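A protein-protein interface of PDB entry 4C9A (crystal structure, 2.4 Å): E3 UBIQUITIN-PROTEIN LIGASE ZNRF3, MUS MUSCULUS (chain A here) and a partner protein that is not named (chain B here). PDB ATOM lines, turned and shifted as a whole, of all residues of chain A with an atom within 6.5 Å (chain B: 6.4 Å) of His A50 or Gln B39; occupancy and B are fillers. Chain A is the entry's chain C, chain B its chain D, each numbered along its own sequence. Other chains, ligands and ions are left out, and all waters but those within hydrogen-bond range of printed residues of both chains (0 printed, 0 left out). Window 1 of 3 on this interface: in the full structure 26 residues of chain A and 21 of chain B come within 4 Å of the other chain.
Of the printed residues of chain B, His A50 touches Asn B19 (3.2 Å), Cys B21 (3.2 Å), Leu B22 (3.9 Å), Phe B30 (3.9 Å), Leu B32 (3.8 Å), Gln B39 (2.6 Å), Tyr B40 (3.9 Å) and Gly B41 (3.4 Å).
Gln B39 touches just these residues of chain A: Gln A48 (3.1 Å), Met A49 (3.5 Å), His A50 (2.6 Å), Gly A53 (3.6 Å) and Tyr A64 (3.8 Å).
Of the printed residues of chain B, Met A49 touches Gln B39 (3.5 Å).
Printed residues of chain A within 4 Å of Tyr B40: His A50 (3.9 Å).
Of the printed residues of chain A, Leu B22 touches His A50 and Leu A52.
Of the printed residues of chain A, Phe B30 touches His A50 (3.9 Å).
Arg A97 touches none of the printed residues of chain B.
The nearest residue of chain B that does not touch His A50 is Gly B20 (5.0 Å).
Printed residues of chain A that touch a printed residue of chain B: Val A47, Gln A48, Met A49, His A50, Pro A51, Leu A52, Gly A53, Tyr A64, Lys A73 and Val A143.
Printed residues of chain B that touch a printed residue of chain A: Asp B18, Asn B19, Cys B21, Leu B22, Phe B30, Leu B32, Arg B34, Met B37, Arg B38, Gln B39, Tyr B40 and Gly B41.
Hydrophobic or aromatic side chains of chain B within 4 Å of the printed part of chain A: Leu B22, Phe B30, Leu B32 and Met B37.
Among the printed residues, Asp or Glu carboxylates within 4 Å of a Lys or Arg side-chain nitrogen of the other chain: Lys A73 with Asp B18 (3.9 Å).
The side-chain amide oxygen (OE1) of Gln B39 is in hydrogen-bond range of the backbone NH (N) of His A50 (2.6 Å).
O of Asp B18 lies within hydrogen-bond range of NE2 of Gln A48 (3.2 Å).
The side-chain amide nitrogen (NE2) of Gln A48 is in hydrogen-bond range of the side-chain amide oxygen (OD1) of Asn B19, at 3.5 Å.
The side-chain amide nitrogen (ND2) of Asn B19 is in hydrogen-bond range of the backbone carbonyl oxygen (O) of Lys A73 (2.9 Å).
OE1 of Gln A48 is in hydrogen-bond range of N of Gln B39 (3.1 Å).
The side-chain amino group (NZ) of Lys A73 is in salt-bridge range of the side-chain carboxylate (OD2) of Asp B18, 3.9 Å away.
The backbone carbonyl oxygen (O) of Gln A48 sits at hydrogen-bond distance from the guanidinium group (NH2) of Arg B34 (2.6 Å).
A ring nitrogen (NE2) of His A50 lies within hydrogen-bond range of the backbone carbonyl oxygen (O) of Cys B21 (3.2 Å).
The side-chain hydroxyl (OH) of Tyr A64 is in hydrogen-bond range of the guanidinium group (NH1) of Arg B34.
NE2 of His A50 lies close to O of Asn B19 (3.4 Å).
N of Gln A48 lies within hydrogen-bond range of O of Met B37.
O of Val A47 sits at hydrogen-bond distance from N of Val A71 (3.0 Å).
The guanidinium group (NH2) of Arg B34 is in hydrogen-bond range of the backbone carbonyl oxygen (O) of Arg B38.
The backbone NH (N) of Cys B21 is in hydrogen-bond range of the backbone carbonyl oxygen (O) of Gly B41 (2.8 Å).
The guanidinium group of Arg B33 lies within hydrogen-bond range of the side-chain hydroxyl of Tyr B40 (2.6 Å).
The backbone carbonyl oxygen (O) of Pro A51 lies within hydrogen-bond range of the side-chain amino group (NZ) of Lys A90, at 3.0 Å.
O of Asn B19 lies within hydrogen-bond range of N of Gly B41.
Among the printed residues, pairs that only touch across the chains: Val A47 with Arg B34, Val A47 with Met B37, Gln A48 with Arg B38, Met A49 with Gln B39, His A50 with Leu B22, His A50 with Phe B30, His A50 with Leu B32, His A50 with Tyr B40, His A50 with Gly B41, Pro A51 with Asn B19, Leu A52 with Leu B22, Gly A53 with Leu B32, Gly A53 with Gln B39, Tyr A64 with Gln B39, Val A143 with Met B37 and Val A143 with Arg B38.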
ATOM      1  N   VAL A  47       8.387  -5.025   6.780  1.00  0.00           N
ATOM      2  CA  VAL A  47       9.035  -5.882   5.779  1.00  0.00           C
ATOM      3  C   VAL A  47       9.463  -5.037   4.592  1.00  0.00           C
ATOM      4  O   VAL A  47       8.646  -4.294   4.059  1.00  0.00           O
ATOM      5  CB  VAL A  47       8.079  -6.944   5.276  1.00  0.00           C
ATOM      6  CG1 VAL A  47       8.786  -7.816   4.259  1.00  0.00           C
ATOM      7  CG2 VAL A  47       7.517  -7.745   6.427  1.00  0.00           C
ATOM      8  N   GLN A  48      10.741  -5.097   4.212  1.00  0.00           N
ATOM      9  CA  GLN A  48      11.245  -4.288   3.099  1.00  0.00           C
ATOM     10  C   GLN A  48      10.902  -5.009   1.853  1.00  0.00           C
ATOM     11  O   GLN A  48      11.026  -6.246   1.802  1.00  0.00           O
ATOM     12  CB  GLN A  48      12.744  -4.114   3.123  1.00  0.00           C
ATOM     13  CG  GLN A  48      13.282  -3.530   1.831  1.00  0.00           C
ATOM     14  CD  GLN A  48      14.808  -3.282   1.827  1.00  0.00           C
ATOM     15  OE1 GLN A  48      15.622  -4.059   2.360  1.00  0.00           O
ATOM     16  NE2 GLN A  48      15.198  -2.237   1.127  1.00  0.00           N
ATOM     17  N   MET A  49      10.413  -4.278   0.851  1.00  0.00           N
ATOM     18  CA  MET A  49      10.257  -4.900  -0.441  1.00  0.00           C
ATOM     19  C   MET A  49      11.152  -4.223  -1.497  1.00  0.00           C
ATOM     20  O   MET A  49      11.280  -3.012  -1.573  1.00  0.00           O
ATOM     21  CB  MET A  49       8.818  -4.913  -0.868  1.00  0.00           C
ATOM     22  CG  MET A  49       7.892  -5.623   0.064  1.00  0.00           C
ATOM     23  SD  MET A  49       7.844  -7.405   0.084  1.00  0.00           S
ATOM     24  CE  MET A  49       7.496  -7.608  -1.653  1.00  0.00           C
ATOM     25  N   HIS A  50      11.857  -5.037  -2.260  1.00  0.00           N
ATOM     26  CA  HIS A  50      12.659  -4.506  -3.346  1.00  0.00           C
ATOM     27  C   HIS A  50      11.601  -4.020  -4.322  1.00  0.00           C
ATOM     28  O   HIS A  50      10.566  -4.644  -4.440  1.00  0.00           O
ATOM     29  CB  HIS A  50      13.548  -5.605  -3.932  1.00  0.00           C
ATOM     30  CG  HIS A  50      14.527  -5.129  -4.959  1.00  0.00           C
ATOM     31  ND1 HIS A  50      14.148  -4.580  -6.166  1.00  0.00           N
ATOM     32  CD2 HIS A  50      15.880  -5.167  -4.977  1.00  0.00           C
ATOM     33  CE1 HIS A  50      15.221  -4.264  -6.865  1.00  0.00           C
ATOM     34  NE2 HIS A  50      16.287  -4.600  -6.157  1.00  0.00           N
ATOM     35  N   PRO A  51      11.847  -2.908  -4.998  1.00  0.00           N
ATOM     36  CA  PRO A  51      10.962  -2.336  -5.989  1.00  0.00           C
ATOM     37  C   PRO A  51      10.455  -3.328  -6.999  1.00  0.00           C
ATOM     38  O   PRO A  51       9.250  -3.432  -7.199  1.00  0.00           O
ATOM     39  CB  PRO A  51      11.850  -1.304  -6.665  1.00  0.00           C
ATOM     40  CG  PRO A  51      12.700  -0.815  -5.572  1.00  0.00           C
ATOM     41  CD  PRO A  51      12.967  -2.000  -4.698  1.00  0.00           C
ATOM     42  N   LEU A  52      11.365  -4.030  -7.653  1.00  0.00           N
ATOM     43  CA  LEU A  52      11.016  -5.218  -8.477  1.00  0.00           C
ATOM     44  C   LEU A  52      10.399  -6.390  -7.669  1.00  0.00           C
ATOM     45  O   LEU A  52       9.976  -7.373  -8.245  1.00  0.00           O
ATOM     46  CB  LEU A  52      12.266  -5.737  -9.210  1.00  0.00           C
ATOM     47  CG  LEU A  52      12.767  -4.938 -10.414  1.00  0.00           C
ATOM     48  CD1 LEU A  52      13.896  -3.973 -10.079  1.00  0.00           C
ATOM     49  CD2 LEU A  52      13.214  -5.920 -11.513  1.00  0.00           C
ATOM     50  N   GLY A  53      10.347  -6.289  -6.342  1.00  0.00           N
ATOM     51  CA  GLY A  53       9.823  -7.372  -5.501  1.00  0.00           C
ATOM     52  C   GLY A  53       8.323  -7.457  -5.558  1.00  0.00           C
ATOM     53  O   GLY A  53       7.731  -8.366  -4.968  1.00  0.00           O
ATOM     54  N   LEU A  54       7.727  -6.498  -6.268  1.00  0.00           N
ATOM     55  CA  LEU A  54       6.299  -6.259  -6.257  1.00  0.00           C
ATOM     56  C   LEU A  54       5.805  -6.175  -7.703  1.00  0.00           C
ATOM     57  O   LEU A  54       5.500  -5.098  -8.210  1.00  0.00           O
ATOM     58  CB  LEU A  54       6.019  -4.946  -5.532  1.00  0.00           C
ATOM     59  CG  LEU A  54       5.760  -4.979  -4.049  1.00  0.00           C
ATOM     60  CD1 LEU A  54       6.048  -3.619  -3.464  1.00  0.00           C
ATOM     61  CD2 LEU A  54       4.327  -5.345  -3.720  1.00  0.00           C
ATOM     62  N   ASP A  62       5.715 -15.840  -2.826  1.00  0.00           N
ATOM     63  CA  ASP A  62       6.034 -16.172  -1.419  1.00  0.00           C
ATOM     64  C   ASP A  62       5.087 -15.441  -0.449  1.00  0.00           C
ATOM     65  O   ASP A  62       4.568 -14.338  -0.751  1.00  0.00           O
ATOM     66  CB  ASP A  62       7.478 -15.785  -1.065  1.00  0.00           C
ATOM     67  CG  ASP A  62       8.515 -16.534  -1.895  1.00  0.00           C
ATOM     68  OD1 ASP A  62       8.471 -17.784  -1.980  1.00  0.00           O
ATOM     69  OD2 ASP A  62       9.394 -15.860  -2.464  1.00  0.00           O
ATOM     70  N   TYR A  64       3.820 -13.638   3.101  1.00  0.00           N
ATOM     71  CA  TYR A  64       4.097 -12.946   4.371  1.00  0.00           C
ATOM     72  C   TYR A  64       2.851 -12.952   5.264  1.00  0.00           C
ATOM     73  O   TYR A  64       1.714 -12.958   4.790  1.00  0.00           O
ATOM     74  CB  TYR A  64       4.637 -11.512   4.138  1.00  0.00           C
ATOM     75  CG  TYR A  64       5.850 -11.482   3.213  1.00  0.00           C
ATOM     76  CD1 TYR A  64       7.132 -11.726   3.707  1.00  0.00           C
ATOM     77  CD2 TYR A  64       5.695 -11.274   1.830  1.00  0.00           C
ATOM     78  CE1 TYR A  64       8.222 -11.750   2.846  1.00  0.00           C
ATOM     79  CE2 TYR A  64       6.775 -11.285   0.960  1.00  0.00           C
ATOM     80  CZ  TYR A  64       8.042 -11.531   1.460  1.00  0.00           C
ATOM     81  OH  TYR A  64       9.148 -11.556   0.617  1.00  0.00           O
ATOM     82  N   VAL A  71       8.000  -1.444   3.287  1.00  0.00           N
ATOM     83  CA  VAL A  71       8.848  -0.295   3.037  1.00  0.00           C
ATOM     84  C   VAL A  71       9.540  -0.483   1.668  1.00  0.00           C
ATOM     85  O   VAL A  71      10.093  -1.550   1.388  1.00  0.00           O
ATOM     86  CB  VAL A  71       9.990  -0.231   4.082  1.00  0.00           C
ATOM     87  CG1 VAL A  71      11.029   0.784   3.689  1.00  0.00           C
ATOM     88  CG2 VAL A  71       9.484   0.065   5.507  1.00  0.00           C
ATOM     89  N   VAL A  72       9.535   0.558   0.840  1.00  0.00           N
ATOM     90  CA  VAL A  72      10.079   0.462  -0.487  1.00  0.00           C
ATOM     91  C   VAL A  72      10.933   1.650  -0.727  1.00  0.00           C
ATOM     92  O   VAL A  72      10.476   2.783  -0.688  1.00  0.00           O
ATOM     93  CB  VAL A  72       8.990   0.440  -1.554  1.00  0.00           C
ATOM     94  CG1 VAL A  72       9.585  -0.019  -2.874  1.00  0.00           C
ATOM     95  CG2 VAL A  72       7.863  -0.506  -1.152  1.00  0.00           C
ATOM     96  N   LYS A  73      12.203   1.368  -0.960  1.00  0.00           N
ATOM     97  CA  LYS A  73      13.122   2.399  -1.326  1.00  0.00           C
ATOM     98  C   LYS A  73      13.042   2.521  -2.836  1.00  0.00           C
ATOM     99  O   LYS A  73      13.480   1.640  -3.539  1.00  0.00           O
ATOM    100  CB  LYS A  73      14.514   2.050  -0.869  1.00  0.00           C
ATOM    101  CG  LYS A  73      15.592   2.809  -1.591  1.00  0.00           C
ATOM    102  CD  LYS A  73      15.496   4.269  -1.275  1.00  0.00           C
ATOM    103  CE  LYS A  73      16.812   4.952  -1.589  1.00  0.00           C
ATOM    104  NZ  LYS A  73      16.723   6.246  -0.888  1.00  0.00           N
ATOM    105  N   LYS A  90       2.225  -0.974  -7.422  1.00  0.00           N
ATOM    106  CA  LYS A  90       3.061  -1.623  -6.435  1.00  0.00           C
ATOM    107  C   LYS A  90       2.422  -1.475  -5.103  1.00  0.00           C
ATOM    108  O   LYS A  90       2.374  -2.457  -4.330  1.00  0.00           O
ATOM    109  CB  LYS A  90       4.424  -1.033  -6.413  1.00  0.00           C
ATOM    110  CG  LYS A  90       5.257  -1.515  -7.610  1.00  0.00           C
ATOM    111  CD  LYS A  90       6.578  -0.740  -7.709  1.00  0.00           C
ATOM    112  CE  LYS A  90       7.277  -0.931  -9.038  1.00  0.00           C
ATOM    113  NZ  LYS A  90       7.454  -2.382  -9.355  1.00  0.00           N
ATOM    114  N   ARG A  97      -1.248  -8.314  -0.901  1.00  0.00           N
ATOM    115  CA  ARG A  97      -0.473  -9.379  -0.242  1.00  0.00           C
ATOM    116  C   ARG A  97      -0.355  -9.144   1.255  1.00  0.00           C
ATOM    117  O   ARG A  97       0.436  -9.775   1.931  1.00  0.00           O
ATOM    118  CB  ARG A  97       0.887  -9.506  -0.869  1.00  0.00           C
ATOM    119  CG  ARG A  97       0.785  -9.767  -2.359  1.00  0.00           C
ATOM    120  CD  ARG A  97       2.100  -9.545  -3.073  1.00  0.00           C
ATOM    121  NE  ARG A  97       3.146 -10.412  -2.532  1.00  0.00           N
ATOM    122  CZ  ARG A  97       4.439 -10.319  -2.820  1.00  0.00           C
ATOM    123  NH1 ARG A  97       4.875  -9.393  -3.664  1.00  0.00           N
ATOM    124  NH2 ARG A  97       5.297 -11.174  -2.260  1.00  0.00           N
ATOM    125  N   VAL A 143      16.400  -0.523   8.980  1.00  0.00           N
ATOM    126  CA  VAL A 143      16.060  -1.657   8.119  1.00  0.00           C
ATOM    127  C   VAL A 143      17.295  -2.458   7.683  1.00  0.00           C
ATOM    128  O   VAL A 143      17.279  -3.689   7.671  1.00  0.00           O
ATOM    129  CB  VAL A 143      15.324  -1.197   6.861  1.00  0.00           C
ATOM    130  CG1 VAL A 143      15.286  -2.314   5.848  1.00  0.00           C
ATOM    131  CG2 VAL A 143      13.907  -0.734   7.220  1.00  0.00           C
ATOM    132  N   ASP B  18      20.786   0.330  -0.546  1.00  0.00           N
ATOM    133  CA  ASP B  18      19.471  -0.049   0.011  1.00  0.00           C
ATOM    134  C   ASP B  18      18.776  -1.210  -0.662  1.00  0.00           C
ATOM    135  O   ASP B  18      18.176  -2.016   0.027  1.00  0.00           O
ATOM    136  CB  ASP B  18      18.524   1.157   0.043  1.00  0.00           C
ATOM    137  CG  ASP B  18      18.890   2.133   1.122  1.00  0.00           C
ATOM    138  OD1 ASP B  18      19.434   1.657   2.162  1.00  0.00           O
ATOM    139  OD2 ASP B  18      18.662   3.354   0.921  1.00  0.00           O
ATOM    140  N   ASN B  19      18.828  -1.294  -1.992  1.00  0.00           N
ATOM    141  CA  ASN B  19      18.259  -2.438  -2.706  1.00  0.00           C
ATOM    142  C   ASN B  19      19.222  -3.471  -3.296  1.00  0.00           C
ATOM    143  O   ASN B  19      18.778  -4.436  -3.906  1.00  0.00           O
ATOM    144  CB  ASN B  19      17.381  -1.926  -3.809  1.00  0.00           C
ATOM    145  CG  ASN B  19      16.181  -1.155  -3.278  1.00  0.00           C
ATOM    146  OD1 ASN B  19      15.585  -1.540  -2.266  1.00  0.00           O
ATOM    147  ND2 ASN B  19      15.799  -0.083  -3.985  1.00  0.00           N
ATOM    148  N   GLY B  20      20.526  -3.290  -3.121  1.00  0.00           N
ATOM    149  CA  GLY B  20      21.493  -4.200  -3.712  1.00  0.00           C
ATOM    150  C   GLY B  20      21.349  -4.085  -5.213  1.00  0.00           C
ATOM    151  O   GLY B  20      21.044  -2.981  -5.729  1.00  0.00           O
ATOM    152  N   CYS B  21      21.533  -5.208  -5.922  1.00  0.00           N
ATOM    153  CA  CYS B  21      21.545  -5.162  -7.386  1.00  0.00           C
ATOM    154  C   CYS B  21      20.163  -4.753  -7.908  1.00  0.00           C
ATOM    155  O   CYS B  21      19.158  -5.258  -7.418  1.00  0.00           O
ATOM    156  CB  CYS B  21      22.014  -6.519  -7.986  1.00  0.00           C
ATOM    157  SG  CYS B  21      23.818  -6.711  -8.085  1.00  0.00           S
ATOM    158  N   LEU B  22      20.114  -3.840  -8.875  1.00  0.00           N
ATOM    159  CA  LEU B  22      18.844  -3.383  -9.506  1.00  0.00           C
ATOM    160  C   LEU B  22      18.627  -3.923 -10.934  1.00  0.00           C
ATOM    161  O   LEU B  22      17.488  -4.017 -11.421  1.00  0.00           O
ATOM    162  CB  LEU B  22      18.786  -1.853  -9.556  1.00  0.00           C
ATOM    163  CG  LEU B  22      18.911  -1.173  -8.192  1.00  0.00           C
ATOM    164  CD1 LEU B  22      19.473   0.235  -8.309  1.00  0.00           C
ATOM    165  CD2 LEU B  22      17.560  -1.147  -7.518  1.00  0.00           C
ATOM    166  N   PHE B  30      18.729 -12.430 -12.062  1.00  0.00           N
ATOM    167  CA  PHE B  30      18.285 -11.576 -10.945  1.00  0.00           C
ATOM    168  C   PHE B  30      17.566 -12.336  -9.820  1.00  0.00           C
ATOM    169  O   PHE B  30      16.576 -13.000 -10.071  1.00  0.00           O
ATOM    170  CB  PHE B  30      17.368 -10.503 -11.453  1.00  0.00           C
ATOM    171  CG  PHE B  30      16.954  -9.539 -10.405  1.00  0.00           C
ATOM    172  CD1 PHE B  30      17.873  -8.640  -9.880  1.00  0.00           C
ATOM    173  CD2 PHE B  30      15.645  -9.525  -9.933  1.00  0.00           C
ATOM    174  CE1 PHE B  30      17.481  -7.724  -8.926  1.00  0.00           C
ATOM    175  CE2 PHE B  30      15.260  -8.625  -8.958  1.00  0.00           C
ATOM    176  CZ  PHE B  30      16.165  -7.712  -8.470  1.00  0.00           C
ATOM    177  N   LEU B  32      15.974 -12.104  -5.718  1.00  0.00           N
ATOM    178  CA  LEU B  32      15.683 -11.400  -4.461  1.00  0.00           C
ATOM    179  C   LEU B  32      16.161 -12.188  -3.259  1.00  0.00           C
ATOM    180  O   LEU B  32      15.670 -13.264  -3.004  1.00  0.00           O
ATOM    181  CB  LEU B  32      14.201 -11.145  -4.326  1.00  0.00           C
ATOM    182  CG  LEU B  32      13.682 -10.278  -5.469  1.00  0.00           C
ATOM    183  CD1 LEU B  32      12.166 -10.147  -5.400  1.00  0.00           C
ATOM    184  CD2 LEU B  32      14.377  -8.913  -5.509  1.00  0.00           C
ATOM    185  N   ARG B  33      17.136 -11.683  -2.517  1.00  0.00           N
ATOM    186  CA  ARG B  33      17.484 -12.364  -1.265  1.00  0.00           C
ATOM    187  C   ARG B  33      16.731 -11.698  -0.094  1.00  0.00           C
ATOM    188  O   ARG B  33      16.623 -10.450  -0.003  1.00  0.00           O
ATOM    189  CB  ARG B  33      18.988 -12.362  -1.038  1.00  0.00           C
ATOM    190  CG  ARG B  33      19.475 -13.256   0.082  1.00  0.00           C
ATOM    191  CD  ARG B  33      20.987 -13.321   0.008  1.00  0.00           C
ATOM    192  NE  ARG B  33      21.544 -14.175   1.038  1.00  0.00           N
ATOM    193  CZ  ARG B  33      21.692 -13.822   2.317  1.00  0.00           C
ATOM    194  NH1 ARG B  33      21.327 -12.612   2.740  1.00  0.00           N
ATOM    195  NH2 ARG B  33      22.212 -14.685   3.184  1.00  0.00           N
ATOM    196  N   ARG B  34      16.174 -12.551   0.760  1.00  0.00           N
ATOM    197  CA  ARG B  34      15.501 -12.139   1.957  1.00  0.00           C
ATOM    198  C   ARG B  34      16.522 -12.345   3.015  1.00  0.00           C
ATOM    199  O   ARG B  34      17.216 -13.370   3.004  1.00  0.00           O
ATOM    200  CB  ARG B  34      14.318 -13.053   2.231  1.00  0.00           C
ATOM    201  CG  ARG B  34      13.417 -12.594   3.377  1.00  0.00           C
ATOM    202  CD  ARG B  34      12.239 -11.765   2.887  1.00  0.00           C
ATOM    203  NE  ARG B  34      12.446 -10.390   3.258  1.00  0.00           N
ATOM    204  CZ  ARG B  34      11.788  -9.350   2.765  1.00  0.00           C
ATOM    205  NH1 ARG B  34      10.838  -9.476   1.840  1.00  0.00           N
ATOM    206  NH2 ARG B  34      12.143  -8.144   3.210  1.00  0.00           N
ATOM    207  N   GLU B  35      16.585 -11.411   3.963  1.00  0.00           N
ATOM    208  CA  GLU B  35      17.608 -11.429   4.990  1.00  0.00           C
ATOM    209  C   GLU B  35      17.096 -10.588   6.137  1.00  0.00           C
ATOM    210  O   GLU B  35      17.414  -9.390   6.248  1.00  0.00           O
ATOM    211  CB  GLU B  35      18.911 -10.874   4.420  1.00  0.00           C
ATOM    212  CG  GLU B  35      20.074 -10.792   5.391  1.00  0.00           C
ATOM    213  CD  GLU B  35      20.438 -12.146   5.960  1.00  0.00           C
ATOM    214  OE1 GLU B  35      20.563 -13.109   5.169  1.00  0.00           O
ATOM    215  OE2 GLU B  35      20.590 -12.245   7.192  1.00  0.00           O
ATOM    216  N   GLY B  36      16.303 -11.216   7.006  1.00  0.00           N
ATOM    217  CA  GLY B  36      15.685 -10.477   8.100  1.00  0.00           C
ATOM    218  C   GLY B  36      14.583  -9.615   7.485  1.00  0.00           C
ATOM    219  O   GLY B  36      13.748 -10.131   6.762  1.00  0.00           O
ATOM    220  N   MET B  37      14.628  -8.308   7.725  1.00  0.00           N
ATOM    221  CA  MET B  37      13.695  -7.371   7.135  1.00  0.00           C
ATOM    222  C   MET B  37      14.016  -7.046   5.695  1.00  0.00           C
ATOM    223  O   MET B  37      13.125  -6.599   4.955  1.00  0.00           O
ATOM    224  CB  MET B  37      13.760  -6.064   7.943  1.00  0.00           C
ATOM    225  CG  MET B  37      12.966  -6.059   9.269  1.00  0.00           C
ATOM    226  SD  MET B  37      13.150  -4.245  10.045  1.00  0.00           S
ATOM    227  CE  MET B  37      14.981  -4.208  10.770  1.00  0.00           C
ATOM    228  N   ARG B  38      15.268  -7.280   5.276  1.00  0.00           N
ATOM    229  CA  ARG B  38      15.756  -6.771   3.995  1.00  0.00           C
ATOM    230  C   ARG B  38      15.339  -7.640   2.854  1.00  0.00           C
ATOM    231  O   ARG B  38      15.136  -8.836   3.032  1.00  0.00           O
ATOM    232  CB  ARG B  38      17.270  -6.658   3.951  1.00  0.00           C
ATOM    233  CG  ARG B  38      17.904  -6.079   5.200  1.00  0.00           C
ATOM    234  CD  ARG B  38      19.395  -5.959   5.013  1.00  0.00           C
ATOM    235  NE  ARG B  38      19.673  -5.334   3.723  1.00  0.00           N
ATOM    236  CZ  ARG B  38      20.826  -5.453   3.083  1.00  0.00           C
ATOM    237  NH1 ARG B  38      21.812  -6.169   3.611  1.00  0.00           N
ATOM    238  NH2 ARG B  38      20.977  -4.850   1.911  1.00  0.00           N
ATOM    239  N   GLN B  39      15.151  -7.004   1.694  1.00  0.00           N
ATOM    240  CA  GLN B  39      14.976  -7.698   0.402  1.00  0.00           C
ATOM    241  C   GLN B  39      15.798  -6.913  -0.576  1.00  0.00           C
ATOM    242  O   GLN B  39      15.449  -5.766  -0.885  1.00  0.00           O
ATOM    243  CB  GLN B  39      13.524  -7.729  -0.090  1.00  0.00           C
ATOM    244  CG  GLN B  39      13.288  -8.715  -1.259  1.00  0.00           C
ATOM    245  CD  GLN B  39      11.909  -8.620  -1.895  1.00  0.00           C
ATOM    246  OE1 GLN B  39      11.456  -7.558  -2.349  1.00  0.00           O
ATOM    247  NE2 GLN B  39      11.229  -9.731  -1.930  1.00  0.00           N
ATOM    248  N   TYR B  40      16.902  -7.504  -1.032  1.00  0.00           N
ATOM    249  CA  TYR B  40      17.770  -6.880  -2.031  1.00  0.00           C
ATOM    250  C   TYR B  40      18.151  -7.824  -3.173  1.00  0.00           C
ATOM    251  O   TYR B  40      18.161  -9.070  -3.048  1.00  0.00           O
ATOM    252  CB  TYR B  40      19.041  -6.344  -1.344  1.00  0.00           C
ATOM    253  CG  TYR B  40      19.790  -7.402  -0.575  1.00  0.00           C
ATOM    254  CD1 TYR B  40      20.682  -8.268  -1.220  1.00  0.00           C
ATOM    255  CD2 TYR B  40      19.585  -7.561   0.762  1.00  0.00           C
ATOM    256  CE1 TYR B  40      21.358  -9.246  -0.526  1.00  0.00           C
ATOM    257  CE2 TYR B  40      20.252  -8.545   1.471  1.00  0.00           C
ATOM    258  CZ  TYR B  40      21.132  -9.380   0.816  1.00  0.00           C
ATOM    259  OH  TYR B  40      21.777 -10.351   1.525  1.00  0.00           O
ATOM    260  N   GLY B  41      18.502  -7.224  -4.293  1.00  0.00           N
ATOM    261  CA  GLY B  41      18.823  -8.004  -5.485  1.00  0.00           C
ATOM    262  C   GLY B  41      20.228  -8.549  -5.469  1.00  0.00           C
ATOM    263  O   GLY B  41      21.167  -7.851  -5.095  1.00  0.00           O
